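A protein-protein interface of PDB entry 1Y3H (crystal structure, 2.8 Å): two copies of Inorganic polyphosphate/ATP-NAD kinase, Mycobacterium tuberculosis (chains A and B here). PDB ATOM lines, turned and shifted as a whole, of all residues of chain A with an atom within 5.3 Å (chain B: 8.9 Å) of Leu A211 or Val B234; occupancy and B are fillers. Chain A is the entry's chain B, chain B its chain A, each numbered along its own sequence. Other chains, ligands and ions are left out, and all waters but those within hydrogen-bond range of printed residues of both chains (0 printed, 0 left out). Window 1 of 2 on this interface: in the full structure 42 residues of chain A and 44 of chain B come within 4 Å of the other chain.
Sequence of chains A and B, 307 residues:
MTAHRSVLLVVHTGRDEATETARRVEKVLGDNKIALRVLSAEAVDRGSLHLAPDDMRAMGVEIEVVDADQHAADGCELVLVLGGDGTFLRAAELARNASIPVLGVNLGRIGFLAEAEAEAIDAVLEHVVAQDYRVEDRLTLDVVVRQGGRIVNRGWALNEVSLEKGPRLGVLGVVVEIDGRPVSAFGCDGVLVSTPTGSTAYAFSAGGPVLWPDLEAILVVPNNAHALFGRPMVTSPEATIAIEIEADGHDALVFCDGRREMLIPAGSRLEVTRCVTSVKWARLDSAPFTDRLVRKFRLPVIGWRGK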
ATOM      1  N   PRO A 196     -12.428   6.402   7.896  1.00  0.00           N
ATOM      2  CA  PRO A 196     -12.352   4.949   8.080  1.00  0.00           C
ATOM      3  C   PRO A 196     -10.892   4.498   8.133  1.00  0.00           C
ATOM      4  O   PRO A 196     -10.535   3.553   8.852  1.00  0.00           O
ATOM      5  CB  PRO A 196     -13.088   4.415   6.858  1.00  0.00           C
ATOM      6  CG  PRO A 196     -14.149   5.455   6.639  1.00  0.00           C
ATOM      7  CD  PRO A 196     -13.393   6.745   6.828  1.00  0.00           C
ATOM      8  N   SER A 199      -9.121   5.604  11.499  1.00  0.00           N
ATOM      9  CA  SER A 199      -9.614   4.864  12.659  1.00  0.00           C
ATOM     10  C   SER A 199      -8.583   4.007  13.377  1.00  0.00           C
ATOM     11  O   SER A 199      -8.781   3.620  14.521  1.00  0.00           O
ATOM     12  CB  SER A 199     -10.790   3.973  12.250  1.00  0.00           C
ATOM     13  OG  SER A 199     -10.358   2.891  11.447  1.00  0.00           O
ATOM     14  N   THR A 200      -7.482   3.699  12.715  1.00  0.00           N
ATOM     15  CA  THR A 200      -6.456   2.858  13.332  1.00  0.00           C
ATOM     16  C   THR A 200      -5.371   3.722  13.940  1.00  0.00           C
ATOM     17  O   THR A 200      -4.415   3.228  14.540  1.00  0.00           O
ATOM     18  CB  THR A 200      -5.831   1.931  12.280  1.00  0.00           C
ATOM     19  OG1 THR A 200      -5.629   2.674  11.060  1.00  0.00           O
ATOM     20  CG2 THR A 200      -6.750   0.730  12.020  1.00  0.00           C
ATOM     21  N   PRO A 209     -13.474   2.582  17.523  1.00  0.00           N
ATOM     22  CA  PRO A 209     -13.720   1.313  16.840  1.00  0.00           C
ATOM     23  C   PRO A 209     -13.011   1.146  15.479  1.00  0.00           C
ATOM     24  O   PRO A 209     -13.053   2.039  14.618  1.00  0.00           O
ATOM     25  CB  PRO A 209     -15.231   1.331  16.667  1.00  0.00           C
ATOM     26  CG  PRO A 209     -15.438   2.772  16.225  1.00  0.00           C
ATOM     27  CD  PRO A 209     -14.522   3.561  17.178  1.00  0.00           C
ATOM     28  N   VAL A 210     -12.396  -0.014  15.283  1.00  0.00           N
ATOM     29  CA  VAL A 210     -11.725  -0.324  14.024  1.00  0.00           C
ATOM     30  C   VAL A 210     -12.670  -0.226  12.824  1.00  0.00           C
ATOM     31  O   VAL A 210     -13.586  -1.030  12.690  1.00  0.00           O
ATOM     32  CB  VAL A 210     -11.187  -1.756  14.011  1.00  0.00           C
ATOM     33  CG1 VAL A 210     -10.729  -2.094  12.605  1.00  0.00           C
ATOM     34  CG2 VAL A 210     -10.057  -1.925  15.037  1.00  0.00           C
ATOM     35  N   LEU A 211     -12.464   0.760  11.962  1.00  0.00           N
ATOM     36  CA  LEU A 211     -13.288   0.886  10.763  1.00  0.00           C
ATOM     37  C   LEU A 211     -12.521   0.214   9.628  1.00  0.00           C
ATOM     38  O   LEU A 211     -11.364  -0.178   9.786  1.00  0.00           O
ATOM     39  CB  LEU A 211     -13.575   2.351  10.414  1.00  0.00           C
ATOM     40  CG  LEU A 211     -14.479   3.152  11.366  1.00  0.00           C
ATOM     41  CD1 LEU A 211     -15.581   3.877  10.569  1.00  0.00           C
ATOM     42  CD2 LEU A 211     -15.084   2.220  12.416  1.00  0.00           C
ATOM     43  N   TRP A 212     -13.175   0.064   8.492  1.00  0.00           N
ATOM     44  CA  TRP A 212     -12.560  -0.589   7.360  1.00  0.00           C
ATOM     45  C   TRP A 212     -12.359   0.432   6.250  1.00  0.00           C
ATOM     46  O   TRP A 212     -13.291   1.161   5.878  1.00  0.00           O
ATOM     47  CB  TRP A 212     -13.447  -1.766   6.894  1.00  0.00           C
ATOM     48  CG  TRP A 212     -12.808  -3.149   7.014  1.00  0.00           C
ATOM     49  CD1 TRP A 212     -12.368  -3.942   5.987  1.00  0.00           C
ATOM     50  CD2 TRP A 212     -12.504  -3.867   8.226  1.00  0.00           C
ATOM     51  NE1 TRP A 212     -11.802  -5.104   6.482  1.00  0.00           N
ATOM     52  CE2 TRP A 212     -11.873  -5.084   7.849  1.00  0.00           C
ATOM     53  CE3 TRP A 212     -12.700  -3.604   9.588  1.00  0.00           C
ATOM     54  CZ2 TRP A 212     -11.437  -6.032   8.788  1.00  0.00           C
ATOM     55  CZ3 TRP A 212     -12.256  -4.558  10.532  1.00  0.00           C
ATOM     56  CH2 TRP A 212     -11.634  -5.754  10.121  1.00  0.00           C
ATOM     57  N   PRO A 213     -11.120   0.493   5.711  1.00  0.00           N
ATOM     58  CA  PRO A 213     -10.603   1.363   4.640  1.00  0.00           C
ATOM     59  C   PRO A 213     -11.529   1.649   3.478  1.00  0.00           C
ATOM     60  O   PRO A 213     -11.597   2.780   3.003  1.00  0.00           O
ATOM     61  CB  PRO A 213      -9.328   0.654   4.192  1.00  0.00           C
ATOM     62  CG  PRO A 213      -9.469  -0.777   4.766  1.00  0.00           C
ATOM     63  CD  PRO A 213     -10.110  -0.517   6.077  1.00  0.00           C
ATOM     64  N   LEU A 215     -14.793   1.364   3.621  1.00  0.00           N
ATOM     65  CA  LEU A 215     -16.042   1.928   4.151  1.00  0.00           C
ATOM     66  C   LEU A 215     -16.121   3.444   3.987  1.00  0.00           C
ATOM     67  O   LEU A 215     -15.130   4.149   4.155  1.00  0.00           O
ATOM     68  CB  LEU A 215     -16.191   1.595   5.640  1.00  0.00           C
ATOM     69  CG  LEU A 215     -17.335   2.327   6.374  1.00  0.00           C
ATOM     70  CD1 LEU A 215     -18.679   1.908   5.780  1.00  0.00           C
ATOM     71  CD2 LEU A 215     -17.289   2.032   7.870  1.00  0.00           C
ATOM     72  N   ALA A 217     -17.695   6.389   5.695  1.00  0.00           N
ATOM     73  CA  ALA A 217     -18.362   6.975   6.842  1.00  0.00           C
ATOM     74  C   ALA A 217     -17.434   7.938   7.588  1.00  0.00           C
ATOM     75  O   ALA A 217     -16.252   8.050   7.264  1.00  0.00           O
ATOM     76  CB  ALA A 217     -18.805   5.849   7.784  1.00  0.00           C
ATOM     77  N   LEU A 219     -16.094   8.989  11.499  1.00  0.00           N
ATOM     78  CA  LEU A 219     -16.004   8.519  12.872  1.00  0.00           C
ATOM     79  C   LEU A 219     -15.690   9.689  13.794  1.00  0.00           C
ATOM     80  O   LEU A 219     -14.655  10.336  13.645  1.00  0.00           O
ATOM     81  CB  LEU A 219     -14.875   7.496  12.998  1.00  0.00           C
ATOM     82  CG  LEU A 219     -14.903   6.433  14.099  1.00  0.00           C
ATOM     83  CD1 LEU A 219     -13.458   6.132  14.525  1.00  0.00           C
ATOM     84  CD2 LEU A 219     -15.715   6.893  15.294  1.00  0.00           C
ATOM     85  N   VAL A 234     -20.660   7.288  14.469  1.00  0.00           N
ATOM     86  CA  VAL A 234     -20.227   7.087  13.110  1.00  0.00           C
ATOM     87  C   VAL A 234     -21.408   7.540  12.274  1.00  0.00           C
ATOM     88  O   VAL A 234     -22.552   7.211  12.564  1.00  0.00           O
ATOM     89  CB  VAL A 234     -19.861   5.599  12.867  1.00  0.00           C
ATOM     90  CG1 VAL A 234     -19.358   5.395  11.445  1.00  0.00           C
ATOM     91  CG2 VAL A 234     -18.775   5.170  13.861  1.00  0.00           C
ATOM     92  N   PHE A 289      -6.756  -5.214   4.164  1.00  0.00           N
ATOM     93  CA  PHE A 289      -6.778  -4.588   5.476  1.00  0.00           C
ATOM     94  C   PHE A 289      -6.823  -5.576   6.640  1.00  0.00           C
ATOM     95  O   PHE A 289      -6.051  -5.456   7.596  1.00  0.00           O
ATOM     96  CB  PHE A 289      -7.957  -3.625   5.585  1.00  0.00           C
ATOM     97  CG  PHE A 289      -8.011  -2.909   6.898  1.00  0.00           C
ATOM     98  CD1 PHE A 289      -6.927  -2.151   7.327  1.00  0.00           C
ATOM     99  CD2 PHE A 289      -9.108  -3.047   7.737  1.00  0.00           C
ATOM    100  CE1 PHE A 289      -6.926  -1.546   8.577  1.00  0.00           C
ATOM    101  CE2 PHE A 289      -9.124  -2.448   8.991  1.00  0.00           C
ATOM    102  CZ  PHE A 289      -8.028  -1.695   9.415  1.00  0.00           C
ATOM    103  N   ILE B 178     -13.651 -11.560   8.375  1.00  0.00           N
ATOM    104  CA  ILE B 178     -14.238 -10.595   7.470  1.00  0.00           C
ATOM    105  C   ILE B 178     -13.622 -10.792   6.086  1.00  0.00           C
ATOM    106  O   ILE B 178     -12.399 -10.891   5.932  1.00  0.00           O
ATOM    107  CB  ILE B 178     -14.025  -9.134   7.957  1.00  0.00           C
ATOM    108  CG1 ILE B 178     -14.731  -8.922   9.307  1.00  0.00           C
ATOM    109  CG2 ILE B 178     -14.605  -8.150   6.926  1.00  0.00           C
ATOM    110  CD1 ILE B 178     -14.173  -9.757  10.455  1.00  0.00           C
ATOM    111  N   SER B 194     -24.922  -6.243  13.676  1.00  0.00           N
ATOM    112  CA  SER B 194     -26.125  -5.470  13.509  1.00  0.00           C
ATOM    113  C   SER B 194     -26.036  -4.386  12.489  1.00  0.00           C
ATOM    114  O   SER B 194     -24.951  -3.978  12.099  1.00  0.00           O
ATOM    115  CB  SER B 194     -26.531  -4.833  14.839  1.00  0.00           C
ATOM    116  OG  SER B 194     -25.700  -3.729  15.140  1.00  0.00           O
ATOM    117  N   THR B 195     -27.213  -3.934  12.078  1.00  0.00           N
ATOM    118  CA  THR B 195     -27.362  -2.849  11.138  1.00  0.00           C
ATOM    119  C   THR B 195     -27.051  -1.575  11.932  1.00  0.00           C
ATOM    120  O   THR B 195     -26.814  -1.638  13.149  1.00  0.00           O
ATOM    121  CB  THR B 195     -28.833  -2.759  10.617  1.00  0.00           C
ATOM    122  OG1 THR B 195     -29.722  -2.387  11.685  1.00  0.00           O
ATOM    123  CG2 THR B 195     -29.267  -4.101  10.045  1.00  0.00           C
ATOM    124  N   PRO B 196     -26.997  -0.411  11.255  1.00  0.00           N
ATOM    125  CA  PRO B 196     -26.719   0.804  12.032  1.00  0.00           C
ATOM    126  C   PRO B 196     -27.891   0.993  13.004  1.00  0.00           C
ATOM    127  O   PRO B 196     -27.696   1.239  14.196  1.00  0.00           O
ATOM    128  CB  PRO B 196     -26.656   1.893  10.955  1.00  0.00           C
ATOM    129  CG  PRO B 196     -26.050   1.150   9.784  1.00  0.00           C
ATOM    130  CD  PRO B 196     -26.831  -0.163   9.805  1.00  0.00           C
ATOM    131  N   SER B 199     -27.648  -0.518  16.332  1.00  0.00           N
ATOM    132  CA  SER B 199     -26.459  -0.174  17.125  1.00  0.00           C
ATOM    133  C   SER B 199     -26.850   0.319  18.506  1.00  0.00           C
ATOM    134  O   SER B 199     -26.104   0.147  19.476  1.00  0.00           O
ATOM    135  CB  SER B 199     -25.620   0.892  16.411  1.00  0.00           C
ATOM    136  OG  SER B 199     -26.378   2.059  16.135  1.00  0.00           O
ATOM    137  N   GLY B 208     -20.903  -1.585  21.763  1.00  0.00           N
ATOM    138  CA  GLY B 208     -20.857  -0.921  20.473  1.00  0.00           C
ATOM    139  C   GLY B 208     -21.037   0.579  20.470  1.00  0.00           C
ATOM    140  O   GLY B 208     -21.552   1.133  21.426  1.00  0.00           O
ATOM    141  N   PRO B 209     -20.596   1.270  19.407  1.00  0.00           N
ATOM    142  CA  PRO B 209     -20.712   2.725  19.267  1.00  0.00           C
ATOM    143  C   PRO B 209     -22.006   3.043  18.543  1.00  0.00           C
ATOM    144  O   PRO B 209     -22.604   2.170  17.914  1.00  0.00           O
ATOM    145  CB  PRO B 209     -19.499   3.077  18.419  1.00  0.00           C
ATOM    146  CG  PRO B 209     -19.456   1.927  17.468  1.00  0.00           C
ATOM    147  CD  PRO B 209     -19.659   0.735  18.399  1.00  0.00           C
ATOM    148  N   VAL B 210     -22.430   4.295  18.610  1.00  0.00           N
ATOM    149  CA  VAL B 210     -23.669   4.693  17.966  1.00  0.00           C
ATOM    150  C   VAL B 210     -23.440   4.928  16.480  1.00  0.00           C
ATOM    151  O   VAL B 210     -22.384   5.398  16.096  1.00  0.00           O
ATOM    152  CB  VAL B 210     -24.215   5.984  18.618  1.00  0.00           C
ATOM    153  CG1 VAL B 210     -25.626   6.265  18.131  1.00  0.00           C
ATOM    154  CG2 VAL B 210     -24.169   5.852  20.127  1.00  0.00           C
ATOM    155  N   LEU B 211     -24.417   4.591  15.646  1.00  0.00           N
ATOM    156  CA  LEU B 211     -24.279   4.798  14.206  1.00  0.00           C
ATOM    157  C   LEU B 211     -25.585   5.370  13.722  1.00  0.00           C
ATOM    158  O   LEU B 211     -26.637   4.807  14.001  1.00  0.00           O
ATOM    159  CB  LEU B 211     -24.024   3.480  13.452  1.00  0.00           C
ATOM    160  CG  LEU B 211     -23.058   2.420  13.985  1.00  0.00           C
ATOM    161  CD1 LEU B 211     -22.809   1.413  12.886  1.00  0.00           C
ATOM    162  CD2 LEU B 211     -21.754   3.041  14.431  1.00  0.00           C
ATOM    163  N   LEU B 215     -26.804   5.710   7.637  1.00  0.00           N
ATOM    164  CA  LEU B 215     -25.516   5.184   7.199  1.00  0.00           C
ATOM    165  C   LEU B 215     -25.657   3.706   6.859  1.00  0.00           C
ATOM    166  O   LEU B 215     -26.393   2.976   7.524  1.00  0.00           O
ATOM    167  CB  LEU B 215     -24.449   5.324   8.290  1.00  0.00           C
ATOM    168  CG  LEU B 215     -23.278   4.343   8.145  1.00  0.00           C
ATOM    169  CD1 LEU B 215     -22.582   4.641   6.851  1.00  0.00           C
ATOM    170  CD2 LEU B 215     -22.305   4.432   9.318  1.00  0.00           C
ATOM    171  N   GLU B 216     -24.940   3.267   5.829  1.00  0.00           N
ATOM    172  CA  GLU B 216     -24.979   1.875   5.424  1.00  0.00           C
ATOM    173  C   GLU B 216     -23.658   1.221   5.703  1.00  0.00           C
ATOM    174  O   GLU B 216     -22.659   1.527   5.073  1.00  0.00           O
ATOM    175  CB  GLU B 216     -25.316   1.772   3.956  1.00  0.00           C
ATOM    176  CG  GLU B 216     -26.667   2.341   3.682  1.00  0.00           C
ATOM    177  CD  GLU B 216     -27.192   1.924   2.348  1.00  0.00           C
ATOM    178  OE1 GLU B 216     -28.373   2.226   2.061  1.00  0.00           O
ATOM    179  OE2 GLU B 216     -26.418   1.298   1.590  1.00  0.00           O
ATOM    180  N   ALA B 217     -23.670   0.313   6.664  1.00  0.00           N
ATOM    181  CA  ALA B 217     -22.475  -0.391   7.075  1.00  0.00           C
ATOM    182  C   ALA B 217     -22.903  -1.572   7.918  1.00  0.00           C
ATOM    183  O   ALA B 217     -24.088  -1.887   8.012  1.00  0.00           O
ATOM    184  CB  ALA B 217     -21.606   0.528   7.893  1.00  0.00           C
ATOM    185  N   ILE B 218     -21.941  -2.210   8.558  1.00  0.00           N
ATOM    186  CA  ILE B 218     -22.245  -3.349   9.383  1.00  0.00           C
ATOM    187  C   ILE B 218     -21.444  -3.316  10.661  1.00  0.00           C
ATOM    188  O   ILE B 218     -20.226  -3.200  10.641  1.00  0.00           O
ATOM    189  CB  ILE B 218     -21.958  -4.645   8.629  1.00  0.00           C
ATOM    190  CG1 ILE B 218     -23.037  -4.841   7.560  1.00  0.00           C
ATOM    191  CG2 ILE B 218     -21.876  -5.827   9.604  1.00  0.00           C
ATOM    192  CD1 ILE B 218     -22.706  -5.863   6.507  1.00  0.00           C
ATOM    193  N   LEU B 219     -22.139  -3.432  11.785  1.00  0.00           N
ATOM    194  CA  LEU B 219     -21.472  -3.417  13.059  1.00  0.00           C
ATOM    195  C   LEU B 219     -21.297  -4.837  13.553  1.00  0.00           C
ATOM    196  O   LEU B 219     -22.212  -5.658  13.467  1.00  0.00           O
ATOM    197  CB  LEU B 219     -22.289  -2.617  14.068  1.00  0.00           C
ATOM    198  CG  LEU B 219     -21.521  -1.892  15.176  1.00  0.00           C
ATOM    199  CD1 LEU B 219     -22.512  -1.615  16.297  1.00  0.00           C
ATOM    200  CD2 LEU B 219     -20.347  -2.710  15.699  1.00  0.00           C
ATOM    201  N   VAL B 220     -20.107  -5.112  14.065  1.00  0.00           N
ATOM    202  CA  VAL B 220     -19.761  -6.409  14.616  1.00  0.00           C
ATOM    203  C   VAL B 220     -19.233  -6.070  15.996  1.00  0.00           C
ATOM    204  O   VAL B 220     -18.238  -5.358  16.107  1.00  0.00           O
ATOM    205  CB  VAL B 220     -18.603  -7.103  13.833  1.00  0.00           C
ATOM    206  CG1 VAL B 220     -18.221  -8.417  14.526  1.00  0.00           C
ATOM    207  CG2 VAL B 220     -18.997  -7.337  12.382  1.00  0.00           C
ATOM    208  N   VAL B 221     -19.884  -6.570  17.043  1.00  0.00           N
ATOM    209  CA  VAL B 221     -19.444  -6.285  18.404  1.00  0.00           C
ATOM    210  C   VAL B 221     -19.160  -7.545  19.192  1.00  0.00           C
ATOM    211  O   VAL B 221     -20.083  -8.272  19.560  1.00  0.00           O
ATOM    212  CB  VAL B 221     -20.510  -5.483  19.190  1.00  0.00           C
ATOM    213  CG1 VAL B 221     -20.009  -5.200  20.604  1.00  0.00           C
ATOM    214  CG2 VAL B 221     -20.832  -4.194  18.481  1.00  0.00           C
ATOM    215  N   PRO B 222     -17.881  -7.832  19.468  1.00  0.00           N
ATOM    216  CA  PRO B 222     -17.666  -9.061  20.246  1.00  0.00           C
ATOM    217  C   PRO B 222     -18.489  -8.928  21.530  1.00  0.00           C
ATOM    218  O   PRO B 222     -18.652  -7.809  22.042  1.00  0.00           O
ATOM    219  CB  PRO B 222     -16.152  -9.050  20.525  1.00  0.00           C
ATOM    220  CG  PRO B 222     -15.580  -8.303  19.342  1.00  0.00           C
ATOM    221  CD  PRO B 222     -16.607  -7.196  19.077  1.00  0.00           C
ATOM    222  N   PHE B 229      -7.732  -7.629  22.406  1.00  0.00           N
ATOM    223  CA  PHE B 229      -8.469  -6.913  21.374  1.00  0.00           C
ATOM    224  C   PHE B 229      -9.892  -7.471  21.280  1.00  0.00           C
ATOM    225  O   PHE B 229     -10.086  -8.655  20.975  1.00  0.00           O
ATOM    226  CB  PHE B 229      -7.790  -7.058  20.010  1.00  0.00           C
ATOM    227  CG  PHE B 229      -8.604  -6.509  18.861  1.00  0.00           C
ATOM    228  CD1 PHE B 229      -8.502  -5.177  18.488  1.00  0.00           C
ATOM    229  CD2 PHE B 229      -9.470  -7.334  18.149  1.00  0.00           C
ATOM    230  CE1 PHE B 229      -9.253  -4.672  17.418  1.00  0.00           C
ATOM    231  CE2 PHE B 229     -10.226  -6.840  17.076  1.00  0.00           C
ATOM    232  CZ  PHE B 229     -10.116  -5.507  16.712  1.00  0.00           C
ATOM    233  N   ARG B 231     -12.570  -4.867  20.441  1.00  0.00           N
ATOM    234  CA  ARG B 231     -13.331  -3.693  20.065  1.00  0.00           C
ATOM    235  C   ARG B 231     -14.272  -3.965  18.922  1.00  0.00           C
ATOM    236  O   ARG B 231     -14.048  -4.859  18.115  1.00  0.00           O
ATOM    237  CB  ARG B 231     -12.389  -2.543  19.659  1.00  0.00           C
ATOM    238  CG  ARG B 231     -10.912  -2.795  19.956  1.00  0.00           C
ATOM    239  CD  ARG B 231     -10.286  -1.726  20.868  1.00  0.00           C
ATOM    240  NE  ARG B 231     -10.372  -0.390  20.281  1.00  0.00           N
ATOM    241  CZ  ARG B 231      -9.573   0.624  20.612  1.00  0.00           C
ATOM    242  NH1 ARG B 231      -8.615   0.454  21.530  1.00  0.00           N
ATOM    243  NH2 ARG B 231      -9.744   1.809  20.032  1.00  0.00           N
ATOM    244  N   PRO B 232     -15.362  -3.199  18.846  1.00  0.00           N
ATOM    245  CA  PRO B 232     -16.316  -3.390  17.756  1.00  0.00           C
ATOM    246  C   PRO B 232     -15.630  -3.056  16.440  1.00  0.00           C
ATOM    247  O   PRO B 232     -14.552  -2.448  16.443  1.00  0.00           O
ATOM    248  CB  PRO B 232     -17.452  -2.414  18.101  1.00  0.00           C
ATOM    249  CG  PRO B 232     -16.812  -1.407  19.014  1.00  0.00           C
ATOM    250  CD  PRO B 232     -15.890  -2.261  19.848  1.00  0.00           C
ATOM    251  N   MET B 233     -16.261  -3.446  15.331  1.00  0.00           N
ATOM    252  CA  MET B 233     -15.724  -3.213  13.998  1.00  0.00           C
ATOM    253  C   MET B 233     -16.837  -2.780  13.073  1.00  0.00           C
ATOM    254  O   MET B 233     -17.953  -3.267  13.185  1.00  0.00           O
ATOM    255  CB  MET B 233     -15.102  -4.495  13.469  1.00  0.00           C
ATOM    256  CG  MET B 233     -13.933  -4.982  14.298  1.00  0.00           C
ATOM    257  SD  MET B 233     -13.600  -6.736  14.057  1.00  0.00           S
ATOM    258  CE  MET B 233     -13.357  -7.319  15.742  1.00  0.00           C
ATOM    259  N   VAL B 234     -16.545  -1.856  12.165  1.00  0.00           N
ATOM    260  CA  VAL B 234     -17.551  -1.398  11.218  1.00  0.00           C
ATOM    261  C   VAL B 234     -17.001  -1.687   9.828  1.00  0.00           C
ATOM    262  O   VAL B 234     -15.858  -1.347   9.509  1.00  0.00           O
ATOM    263  CB  VAL B 234     -17.837   0.113  11.338  1.00  0.00           C
ATOM    264  CG1 VAL B 234     -19.145   0.441  10.610  1.00  0.00           C
ATOM    265  CG2 VAL B 234     -17.898   0.525  12.797  1.00  0.00           C
ATOM    266  N   THR B 235     -17.834  -2.314   9.005  1.00  0.00           N
ATOM    267  CA  THR B 235     -17.455  -2.717   7.659  1.00  0.00           C
ATOM    268  C   THR B 235     -18.367  -2.104   6.630  1.00  0.00           C
ATOM    269  O   THR B 235     -19.245  -1.310   6.951  1.00  0.00           O
ATOM    270  CB  THR B 235     -17.572  -4.247   7.478  1.00  0.00           C
ATOM    271  OG1 THR B 235     -18.963  -4.620   7.463  1.00  0.00           O
ATOM    272  CG2 THR B 235     -16.859  -4.972   8.593  1.00  0.00           C
ATOM    273  N   SER B 236     -18.145  -2.515   5.387  1.00  0.00           N
ATOM    274  CA  SER B 236     -18.923  -2.077   4.253  1.00  0.00           C
ATOM    275  C   SER B 236     -20.225  -2.892   4.187  1.00  0.00           C
ATOM    276  O   SER B 236     -20.353  -3.952   4.813  1.00  0.00           O
ATOM    277  CB  SER B 236     -18.096  -2.302   2.989  1.00  0.00           C
ATOM    278  OG  SER B 236     -18.873  -2.153   1.809  1.00  0.00           O
ATOM    279  N   PRO B 237     -21.220  -2.386   3.452  1.00  0.00           N
ATOM    280  CA  PRO B 237     -22.514  -3.055   3.284  1.00  0.00           C
ATOM    281  C   PRO B 237     -22.333  -4.291   2.399  1.00  0.00           C
ATOM    282  O   PRO B 237     -23.246  -5.106   2.261  1.00  0.00           O
ATOM    283  CB  PRO B 237     -23.366  -2.008   2.569  1.00  0.00           C
ATOM    284  CG  PRO B 237     -22.746  -0.711   2.950  1.00  0.00           C
ATOM    285  CD  PRO B 237     -21.268  -1.010   2.935  1.00  0.00           C
ATOM    286  N   ALA B 239     -19.300  -6.083   2.638  1.00  0.00           N
ATOM    287  CA  ALA B 239     -18.379  -6.975   3.308  1.00  0.00           C
ATOM    288  C   ALA B 239     -19.170  -8.228   3.648  1.00  0.00           C
ATOM    289  O   ALA B 239     -20.403  -8.237   3.620  1.00  0.00           O
ATOM    290  CB  ALA B 239     -17.834  -6.341   4.560  1.00  0.00           C
ATOM    291  N   ILE B 241     -19.477 -10.970   6.592  1.00  0.00           N
ATOM    292  CA  ILE B 241     -19.093 -11.373   7.932  1.00  0.00           C
ATOM    293  C   ILE B 241     -19.463 -12.823   8.207  1.00  0.00           C
ATOM    294  O   ILE B 241     -20.603 -13.246   7.983  1.00  0.00           O
ATOM    295  CB  ILE B 241     -19.759 -10.449   9.003  1.00  0.00           C
ATOM    296  CG1 ILE B 241     -19.389  -8.977   8.743  1.00  0.00           C
ATOM    297  CG2 ILE B 241     -19.308 -10.869  10.401  1.00  0.00           C
ATOM    298  CD1 ILE B 241     -20.145  -8.322   7.576  1.00  0.00           C
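The backbone carbonyl oxygen (O) of Val B210 lies within hydrogen-bond range of the backbone NH (N) of Val A234 (3.0 Å). O of Pro B232 is in hydrogen-bond range of N of Val A210. N of Val B234 lies within hydrogen-bond range of O of Val A210 (3.1 Å). The backbone NH of Trp A212 sits at hydrogen-bond distance from the backbone carbonyl oxygen of Val B234, 3.2 Å away.
N of Leu B211 sits at hydrogen-bond distance from OG of Ser B199, 3.2 Å away. The backbone carbonyl oxygen (O) of Ile B218 lies within hydrogen-bond range of the backbone NH (N) of Thr B235. The backbone carbonyl oxygen (O) of Val B220 is in hydrogen-bond range of the backbone NH (N) of Met B233, 2.9 Å away. The side-chain hydroxyl of Ser A199 sits at hydrogen-bond distance from the backbone NH of Leu A211 (3.0 Å).
CB of Pro A209 touches O of Pro B232, 3.8 Å away. Val A210 touches Phe B229 (CG2 to CE1, 3.7 Å). O of Val A210 touches CA of Met B233 (3.3 Å). Val B234 touches Leu A211. Ala B217 touches Leu A215 (CB to CD1, 3.9 Å). Leu A215 touches Val B234. Thr B235 touches Leu A215 (O to CD1, 3.5 Å). CA of Leu B211 touches O of Val A234, 3.4 Å away. Val A234 touches Leu B215 (CG1 to CD2, 3.8 Å).
Val B234 touches just these residues of chain A: Val A210 (3.1 Å), Leu A211 (3.3 Å), Trp A212 (3.2 Å) and Leu A215 (3.7 Å). Of chain B, only Phe B229 (3.7 Å), Pro B232 (3.5 Å), Met B233 (3.3 Å) and Val B234 (3.1 Å) come within 4 Å of Val A210. Of the printed residues of chain B, Leu A215 touches Ala B217 (3.9 Å), Val B234 (3.7 Å) and Thr B235 (3.5 Å). Printed residues of chain A within 4 Å of Phe B229: Val A210 (3.7 Å). Ile B241 touches none of the printed residues of chain A. The nearest printed residue of chain A that does not touch Leu B211 is Pro A209 (6.6 Å).
Printed residues of chain A that touch a printed residue of chain B: Pro A209, Val A210, Leu A211, Trp A212, Leu A215 and Val A234. Among the printed residues, 13 pairs touch across the chains. Among the printed residues, no Asp or Glu carboxylate lies within 4 Å of a Lys or Arg side-chain nitrogen of the other chain.
Val A210 touches Val B234, and with the chains exchanged Val A234 touches Val B210. Leu A211 touches Val B234, and with the chains exchanged Val A234 touches Leu B211. Leu A215 touches Ala B217, but with the chains exchanged Ala A217 does not touch Leu B215 (4.1 Å). Leu A215 touches Val B234, and with the chains exchanged Val A234 touches Leu B215. Positions printed for both chains: 196, 199, 209, 210, 211, 215, 217, 219 and 234. Of the 13 pairs that touch across the chains among the printed residues, 6 have their exchanged pair printed and touching as well.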
